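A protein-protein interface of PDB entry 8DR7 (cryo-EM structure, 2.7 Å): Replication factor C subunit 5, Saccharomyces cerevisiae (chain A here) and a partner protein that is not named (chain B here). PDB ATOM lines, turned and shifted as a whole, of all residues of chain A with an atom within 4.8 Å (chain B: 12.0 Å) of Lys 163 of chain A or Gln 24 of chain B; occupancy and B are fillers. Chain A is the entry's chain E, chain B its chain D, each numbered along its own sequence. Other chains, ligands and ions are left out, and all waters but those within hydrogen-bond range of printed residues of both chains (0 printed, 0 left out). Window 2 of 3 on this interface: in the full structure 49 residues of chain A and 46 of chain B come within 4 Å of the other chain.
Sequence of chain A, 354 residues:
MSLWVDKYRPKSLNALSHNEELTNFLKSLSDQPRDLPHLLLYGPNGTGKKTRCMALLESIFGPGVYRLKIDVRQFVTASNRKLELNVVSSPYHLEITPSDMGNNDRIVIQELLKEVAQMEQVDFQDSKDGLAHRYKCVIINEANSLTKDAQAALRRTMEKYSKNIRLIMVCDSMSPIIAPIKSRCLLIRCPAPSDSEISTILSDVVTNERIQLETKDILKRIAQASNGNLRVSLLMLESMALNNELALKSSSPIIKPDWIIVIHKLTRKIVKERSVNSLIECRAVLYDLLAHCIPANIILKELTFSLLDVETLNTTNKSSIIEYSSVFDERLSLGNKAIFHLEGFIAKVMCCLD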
ATOM      1  N   ARG A  34      -1.930   3.530 -24.479  1.00  0.00           N
ATOM      2  CA  ARG A  34      -0.476   3.656 -24.458  1.00  0.00           C
ATOM      3  C   ARG A  34       0.190   2.321 -24.144  1.00  0.00           C
ATOM      4  O   ARG A  34       1.209   1.970 -24.753  1.00  0.00           O
ATOM      5  CB  ARG A  34      -0.056   4.717 -23.441  1.00  0.00           C
ATOM      6  CG  ARG A  34       0.564   5.956 -24.069  1.00  0.00           C
ATOM      7  CD  ARG A  34       0.611   7.120 -23.088  1.00  0.00           C
ATOM      8  NE  ARG A  34       0.932   8.385 -23.740  1.00  0.00           N
ATOM      9  CZ  ARG A  34       0.155   8.998 -24.625  1.00  0.00           C
ATOM     10  NH1 ARG A  34      -1.023   8.507 -24.971  1.00  0.00           N
ATOM     11  NH2 ARG A  34       0.570  10.137 -25.171  1.00  0.00           N
ATOM     12  N   TYR A 135       2.980   5.033 -31.376  1.00  0.00           N
ATOM     13  CA  TYR A 135       3.280   3.763 -32.019  1.00  0.00           C
ATOM     14  C   TYR A 135       2.383   3.561 -33.235  1.00  0.00           C
ATOM     15  O   TYR A 135       1.372   4.245 -33.415  1.00  0.00           O
ATOM     16  CB  TYR A 135       3.106   2.600 -31.038  1.00  0.00           C
ATOM     17  CG  TYR A 135       1.716   2.485 -30.451  1.00  0.00           C
ATOM     18  CD1 TYR A 135       0.719   1.774 -31.107  1.00  0.00           C
ATOM     19  CD2 TYR A 135       1.401   3.080 -29.237  1.00  0.00           C
ATOM     20  CE1 TYR A 135      -0.550   1.666 -30.575  1.00  0.00           C
ATOM     21  CE2 TYR A 135       0.135   2.975 -28.696  1.00  0.00           C
ATOM     22  CZ  TYR A 135      -0.837   2.267 -29.369  1.00  0.00           C
ATOM     23  OH  TYR A 135      -2.100   2.161 -28.834  1.00  0.00           O
ATOM     24  N   TYR A 161      10.823  -4.483 -30.439  1.00  0.00           N
ATOM     25  CA  TYR A 161      10.238  -3.199 -30.812  1.00  0.00           C
ATOM     26  C   TYR A 161       8.836  -3.067 -30.226  1.00  0.00           C
ATOM     27  O   TYR A 161       7.905  -2.650 -30.922  1.00  0.00           O
ATOM     28  CB  TYR A 161      10.174  -3.046 -32.333  1.00  0.00           C
ATOM     29  CG  TYR A 161      11.463  -3.367 -33.045  1.00  0.00           C
ATOM     30  CD1 TYR A 161      12.591  -2.577 -32.874  1.00  0.00           C
ATOM     31  CD2 TYR A 161      11.549  -4.458 -33.895  1.00  0.00           C
ATOM     32  CE1 TYR A 161      13.770  -2.868 -33.529  1.00  0.00           C
ATOM     33  CE2 TYR A 161      12.721  -4.759 -34.551  1.00  0.00           C
ATOM     34  CZ  TYR A 161      13.828  -3.962 -34.366  1.00  0.00           C
ATOM     35  OH  TYR A 161      14.999  -4.266 -35.021  1.00  0.00           O
ATOM     36  N   SER A 162       8.677  -3.418 -28.948  1.00  0.00           N
ATOM     37  CA  SER A 162       7.339  -3.494 -28.366  1.00  0.00           C
ATOM     38  C   SER A 162       6.638  -2.141 -28.384  1.00  0.00           C
ATOM     39  O   SER A 162       5.458  -2.053 -28.741  1.00  0.00           O
ATOM     40  CB  SER A 162       7.422  -4.030 -26.936  1.00  0.00           C
ATOM     41  OG  SER A 162       8.462  -3.394 -26.212  1.00  0.00           O
ATOM     42  N   LYS A 163       7.341  -1.077 -28.003  1.00  0.00           N
ATOM     43  CA  LYS A 163       6.722   0.232 -27.848  1.00  0.00           C
ATOM     44  C   LYS A 163       6.792   1.087 -29.108  1.00  0.00           C
ATOM     45  O   LYS A 163       6.314   2.226 -29.090  1.00  0.00           O
ATOM     46  CB  LYS A 163       7.364   0.981 -26.673  1.00  0.00           C
ATOM     47  CG  LYS A 163       8.738   1.564 -26.958  1.00  0.00           C
ATOM     48  CD  LYS A 163       8.671   3.073 -27.130  1.00  0.00           C
ATOM     49  CE  LYS A 163      10.048   3.698 -27.049  1.00  0.00           C
ATOM     50  NZ  LYS A 163      10.020   5.167 -27.290  1.00  0.00           N
ATOM     51  N   ASN A 164       7.372   0.575 -30.192  1.00  0.00           N
ATOM     52  CA  ASN A 164       7.356   1.265 -31.476  1.00  0.00           C
ATOM     53  C   ASN A 164       6.302   0.725 -32.429  1.00  0.00           C
ATOM     54  O   ASN A 164       5.748   1.494 -33.221  1.00  0.00           O
ATOM     55  CB  ASN A 164       8.730   1.167 -32.153  1.00  0.00           C
ATOM     56  CG  ASN A 164       9.380   2.523 -32.371  1.00  0.00           C
ATOM     57  OD1 ASN A 164       8.820   3.564 -32.023  1.00  0.00           O
ATOM     58  ND2 ASN A 164      10.570   2.516 -32.959  1.00  0.00           N
ATOM     59  N   ILE A 165       6.014  -0.574 -32.372  1.00  0.00           N
ATOM     60  CA  ILE A 165       5.041  -1.206 -33.252  1.00  0.00           C
ATOM     61  C   ILE A 165       4.164  -2.136 -32.425  1.00  0.00           C
ATOM     62  O   ILE A 165       4.631  -2.797 -31.492  1.00  0.00           O
ATOM     63  CB  ILE A 165       5.730  -1.973 -34.407  1.00  0.00           C
ATOM     64  CG1 ILE A 165       4.958  -1.780 -35.715  1.00  0.00           C
ATOM     65  CG2 ILE A 165       5.877  -3.458 -34.083  1.00  0.00           C
ATOM     66  CD1 ILE A 165       5.764  -2.117 -36.950  1.00  0.00           C
ATOM     67  N   ARG A 166       2.879  -2.176 -32.773  1.00  0.00           N
ATOM     68  CA  ARG A 166       1.911  -3.051 -32.124  1.00  0.00           C
ATOM     69  C   ARG A 166       1.195  -3.858 -33.195  1.00  0.00           C
ATOM     70  O   ARG A 166       0.817  -3.312 -34.237  1.00  0.00           O
ATOM     71  CB  ARG A 166       0.905  -2.247 -31.294  1.00  0.00           C
ATOM     72  CG  ARG A 166       1.536  -1.448 -30.161  1.00  0.00           C
ATOM     73  CD  ARG A 166       2.026  -2.349 -29.038  1.00  0.00           C
ATOM     74  NE  ARG A 166       2.886  -1.638 -28.098  1.00  0.00           N
ATOM     75  CZ  ARG A 166       2.450  -0.840 -27.133  1.00  0.00           C
ATOM     76  NH1 ARG A 166       1.159  -0.613 -26.953  1.00  0.00           N
ATOM     77  NH2 ARG A 166       3.331  -0.255 -26.328  1.00  0.00           N
ATOM     78  N   LEU B  22       8.663   1.768 -18.404  1.00  0.00           N
ATOM     79  CA  LEU B  22       7.916   3.021 -18.391  1.00  0.00           C
ATOM     80  C   LEU B  22       6.420   2.760 -18.520  1.00  0.00           C
ATOM     81  O   LEU B  22       5.984   1.611 -18.585  1.00  0.00           O
ATOM     82  CB  LEU B  22       8.390   3.938 -19.520  1.00  0.00           C
ATOM     83  N   ALA B  23       5.635   3.838 -18.555  1.00  0.00           N
ATOM     84  CA  ALA B  23       4.188   3.723 -18.679  1.00  0.00           C
ATOM     85  C   ALA B  23       3.733   3.440 -20.103  1.00  0.00           C
ATOM     86  O   ALA B  23       2.559   3.112 -20.305  1.00  0.00           O
ATOM     87  CB  ALA B  23       3.518   5.004 -18.176  1.00  0.00           C
ATOM     88  N   GLN B  24       4.623   3.557 -21.091  1.00  0.00           N
ATOM     89  CA  GLN B  24       4.291   3.316 -22.488  1.00  0.00           C
ATOM     90  C   GLN B  24       4.771   1.950 -22.969  1.00  0.00           C
ATOM     91  O   GLN B  24       5.026   1.768 -24.165  1.00  0.00           O
ATOM     92  CB  GLN B  24       4.879   4.420 -23.368  1.00  0.00           C
ATOM     93  CG  GLN B  24       4.547   5.828 -22.902  1.00  0.00           C
ATOM     94  CD  GLN B  24       5.585   6.388 -21.950  1.00  0.00           C
ATOM     95  OE1 GLN B  24       6.776   6.420 -22.259  1.00  0.00           O
ATOM     96  NE2 GLN B  24       5.138   6.837 -20.783  1.00  0.00           N
ATOM     97  N   GLN B  25       4.902   0.987 -22.062  1.00  0.00           N
ATOM     98  CA  GLN B  25       5.349  -0.352 -22.404  1.00  0.00           C
ATOM     99  C   GLN B  25       4.398  -1.385 -21.817  1.00  0.00           C
ATOM    100  O   GLN B  25       3.794  -1.150 -20.766  1.00  0.00           O
ATOM    101  CB  GLN B  25       6.768  -0.614 -21.878  1.00  0.00           C
ATOM    102  CG  GLN B  25       7.842   0.239 -22.532  1.00  0.00           C
ATOM    103  CD  GLN B  25       9.222  -0.032 -21.968  1.00  0.00           C
ATOM    104  OE1 GLN B  25       9.381  -0.821 -21.036  1.00  0.00           O
ATOM    105  NE2 GLN B  25      10.232   0.623 -22.531  1.00  0.00           N
ATOM    106  N   PRO B  26       4.245  -2.536 -22.471  1.00  0.00           N
ATOM    107  CA  PRO B  26       3.443  -3.609 -21.877  1.00  0.00           C
ATOM    108  C   PRO B  26       4.075  -4.131 -20.597  1.00  0.00           C
ATOM    109  O   PRO B  26       5.293  -4.073 -20.407  1.00  0.00           O
ATOM    110  CB  PRO B  26       3.423  -4.690 -22.967  1.00  0.00           C
ATOM    111  CG  PRO B  26       3.733  -3.967 -24.230  1.00  0.00           C
ATOM    112  CD  PRO B  26       4.675  -2.873 -23.840  1.00  0.00           C
ATOM    113  N   TRP B  27       3.223  -4.646 -19.708  1.00  0.00           N
ATOM    114  CA  TRP B  27       3.714  -5.153 -18.430  1.00  0.00           C
ATOM    115  C   TRP B  27       4.713  -6.285 -18.622  1.00  0.00           C
ATOM    116  O   TRP B  27       5.635  -6.442 -17.812  1.00  0.00           O
ATOM    117  CB  TRP B  27       2.544  -5.625 -17.566  1.00  0.00           C
ATOM    118  CG  TRP B  27       1.664  -4.515 -17.075  1.00  0.00           C
ATOM    119  CD1 TRP B  27       1.694  -3.208 -17.466  1.00  0.00           C
ATOM    120  CD2 TRP B  27       0.622  -4.615 -16.096  1.00  0.00           C
ATOM    121  NE1 TRP B  27       0.736  -2.490 -16.794  1.00  0.00           N
ATOM    122  CE2 TRP B  27       0.064  -3.330 -15.947  1.00  0.00           C
ATOM    123  CE3 TRP B  27       0.107  -5.667 -15.333  1.00  0.00           C
ATOM    124  CZ2 TRP B  27      -0.983  -3.069 -15.066  1.00  0.00           C
ATOM    125  CZ3 TRP B  27      -0.932  -5.406 -14.459  1.00  0.00           C
ATOM    126  CH2 TRP B  27      -1.466  -4.118 -14.333  1.00  0.00           C
ATOM    127  N   VAL B  28       4.554  -7.083 -19.679  1.00  0.00           N
ATOM    128  CA  VAL B  28       5.493  -8.172 -19.926  1.00  0.00           C
ATOM    129  C   VAL B  28       6.884  -7.620 -20.214  1.00  0.00           C
ATOM    130  O   VAL B  28       7.891  -8.173 -19.757  1.00  0.00           O
ATOM    131  CB  VAL B  28       4.989  -9.074 -21.069  1.00  0.00           C
ATOM    132  CG1 VAL B  28       3.716  -9.798 -20.651  1.00  0.00           C
ATOM    133  CG2 VAL B  28       4.763  -8.274 -22.347  1.00  0.00           C
ATOM    134  N   GLU B  29       6.966  -6.527 -20.973  1.00  0.00           N
ATOM    135  CA  GLU B  29       8.247  -5.883 -21.241  1.00  0.00           C
ATOM    136  C   GLU B  29       8.672  -4.938 -20.127  1.00  0.00           C
ATOM    137  O   GLU B  29       9.871  -4.815 -19.853  1.00  0.00           O
ATOM    138  CB  GLU B  29       8.192  -5.107 -22.561  1.00  0.00           C
ATOM    139  CG  GLU B  29       7.583  -5.873 -23.726  1.00  0.00           C
ATOM    140  CD  GLU B  29       8.503  -6.957 -24.256  1.00  0.00           C
ATOM    141  OE1 GLU B  29       8.061  -7.742 -25.120  1.00  0.00           O
ATOM    142  OE2 GLU B  29       9.667  -7.023 -23.809  1.00  0.00           O
ATOM    143  N   LYS B  30       7.717  -4.265 -19.478  1.00  0.00           N
ATOM    144  CA  LYS B  30       8.065  -3.335 -18.410  1.00  0.00           C
ATOM    145  C   LYS B  30       8.733  -4.056 -17.246  1.00  0.00           C
ATOM    146  O   LYS B  30       9.709  -3.557 -16.673  1.00  0.00           O
ATOM    147  CB  LYS B  30       6.814  -2.593 -17.938  1.00  0.00           C
ATOM    148  CG  LYS B  30       6.995  -1.797 -16.651  1.00  0.00           C
ATOM    149  CD  LYS B  30       5.727  -1.041 -16.285  1.00  0.00           C
ATOM    150  CE  LYS B  30       5.923  -0.203 -15.032  1.00  0.00           C
ATOM    151  NZ  LYS B  30       4.791   0.738 -14.805  1.00  0.00           N
ATOM    152  N   TYR B  31       8.223  -5.234 -16.883  1.00  0.00           N
ATOM    153  CA  TYR B  31       8.740  -6.005 -15.763  1.00  0.00           C
ATOM    154  C   TYR B  31       9.679  -7.123 -16.207  1.00  0.00           C
ATOM    155  O   TYR B  31       9.828  -8.119 -15.492  1.00  0.00           O
ATOM    156  CB  TYR B  31       7.581  -6.576 -14.944  1.00  0.00           C
ATOM    157  CG  TYR B  31       6.799  -5.519 -14.206  1.00  0.00           C
ATOM    158  CD1 TYR B  31       7.292  -4.957 -13.036  1.00  0.00           C
ATOM    159  CD2 TYR B  31       5.577  -5.065 -14.685  1.00  0.00           C
ATOM    160  CE1 TYR B  31       6.587  -3.988 -12.356  1.00  0.00           C
ATOM    161  CE2 TYR B  31       4.864  -4.092 -14.012  1.00  0.00           C
ATOM    162  CZ  TYR B  31       5.376  -3.556 -12.848  1.00  0.00           C
ATOM    163  OH  TYR B  31       4.676  -2.586 -12.167  1.00  0.00           O
ATOM    164  N   ARG B  32      10.310  -6.979 -17.367  1.00  0.00           N
ATOM    165  CA  ARG B  32      11.305  -7.955 -17.785  1.00  0.00           C
ATOM    166  C   ARG B  32      12.497  -7.909 -16.829  1.00  0.00           C
ATOM    167  O   ARG B  32      12.942  -6.822 -16.446  1.00  0.00           O
ATOM    168  CB  ARG B  32      11.766  -7.672 -19.216  1.00  0.00           C
ATOM    169  CG  ARG B  32      12.937  -8.529 -19.683  1.00  0.00           C
ATOM    170  CD  ARG B  32      13.329  -8.192 -21.112  1.00  0.00           C
ATOM    171  NE  ARG B  32      12.307  -8.601 -22.068  1.00  0.00           N
ATOM    172  CZ  ARG B  32      12.161  -9.834 -22.533  1.00  0.00           C
ATOM    173  NH1 ARG B  32      12.952 -10.819 -22.144  1.00  0.00           N
ATOM    174  NH2 ARG B  32      11.191 -10.086 -23.409  1.00  0.00           N
ATOM    175  N   GLU B 208       1.644  -2.494  -9.417  1.00  0.00           N
ATOM    176  CA  GLU B 208       0.586  -1.882 -10.208  1.00  0.00           C
ATOM    177  C   GLU B 208      -0.661  -1.563  -9.392  1.00  0.00           C
ATOM    178  O   GLU B 208      -1.640  -1.064  -9.956  1.00  0.00           O
ATOM    179  CB  GLU B 208       0.207  -2.799 -11.378  1.00  0.00           C
ATOM    180  CG  GLU B 208       1.311  -3.014 -12.409  1.00  0.00           C
ATOM    181  CD  GLU B 208       1.845  -1.719 -12.999  1.00  0.00           C
ATOM    182  OE1 GLU B 208       2.879  -1.769 -13.699  1.00  0.00           O
ATOM    183  OE2 GLU B 208       1.224  -0.657 -12.788  1.00  0.00           O
ATOM    184  N   GLN B 236      -2.775  -7.939 -16.669  1.00  0.00           N
ATOM    185  CA  GLN B 236      -2.895  -6.596 -17.227  1.00  0.00           C
ATOM    186  C   GLN B 236      -4.286  -6.362 -17.800  1.00  0.00           C
ATOM    187  O   GLN B 236      -4.875  -5.291 -17.605  1.00  0.00           O
ATOM    188  CB  GLN B 236      -1.830  -6.378 -18.302  1.00  0.00           C
ATOM    189  CG  GLN B 236      -1.784  -4.960 -18.849  1.00  0.00           C
ATOM    190  CD  GLN B 236      -0.706  -4.775 -19.899  1.00  0.00           C
ATOM    191  OE1 GLN B 236       0.168  -5.626 -20.064  1.00  0.00           O
ATOM    192  NE2 GLN B 236      -0.764  -3.660 -20.617  1.00  0.00           N
ATOM    193  N   LYS B 240      -6.960  -3.596 -16.511  1.00  0.00           N
ATOM    194  CA  LYS B 240      -7.566  -2.619 -17.410  1.00  0.00           C
ATOM    195  C   LYS B 240      -9.085  -2.664 -17.318  1.00  0.00           C
ATOM    196  O   LYS B 240      -9.745  -1.618 -17.273  1.00  0.00           O
ATOM    197  CB  LYS B 240      -7.112  -2.875 -18.846  1.00  0.00           C
ATOM    198  CG  LYS B 240      -5.768  -2.258 -19.194  1.00  0.00           C
ATOM    199  CD  LYS B 240      -5.269  -2.748 -20.544  1.00  0.00           C
ATOM    200  CE  LYS B 240      -4.046  -1.971 -21.002  1.00  0.00           C
ATOM    201  NZ  LYS B 240      -4.400  -0.607 -21.486  1.00  0.00           N
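The guanidinium group of Arg 32 of chain B lies within salt-bridge range of the side-chain carboxylate of Glu 29 of chain B, at 3.4 Å.
O of Arg 34 of chain A lies within hydrogen-bond range of NH1 of Arg 166 of chain A (3.4 Å).
O of Ser 162 of chain A sits at hydrogen-bond distance from NE of Arg 166 of chain A.
The guanidinium group (NH2) of Arg 166 of chain A sits at hydrogen-bond distance from the backbone carbonyl oxygen (O) of Gln 24 of chain B, 3.4 Å away.
Of the printed residues of chain B, Arg 34 of chain A touches Gln 24 (3.9 Å).
Lys 163 of chain A touches just one residue of chain B: Gln 24.
Gln 24 of chain B touches just these residues of chain A: Arg 34 (3.9 Å), Lys 163 (3.5 Å) and Arg 166 (3.4 Å).
Of the printed residues of chain A, Pro 26 of chain B touches Arg 166.
Printed residues of chain A within 4 Å of Glu 29 of chain B: Ser 162.
Tyr 31 of chain B touches none of the printed residues of chain A.
The nearest residue of chain B that does not touch Lys 163 of chain A is Gln 25 of chain B (4.2 Å).
The nearest printed residue of chain A that does not touch Gln 24 of chain B is Ser 162 of chain A (6.0 Å).
The nearest printed residue of chain A that does not touch Glu 29 of chain B is Lys 163 of chain A (6.4 Å).
Among the printed residues, merely in contact across the chains: Lys 163 of chain A with Gln 24 of chain B, Ser 162 of chain A with Glu 29 of chain B, Arg 166 of chain A with Pro 26 of chain B and Arg 34 of chain A with Gln 24 of chain B.
Printed residues of chain B that touch a printed residue of chain A: Gln 24, Pro 26 and Glu 29.
Hydrophobic or aromatic side chains of chain B that line the printed part of chain A: Pro 26.
Of the 8 printed residues of chain A, 4 touch a printed residue of chain B.
Among the printed residues, 5 pairs touch across the chains.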
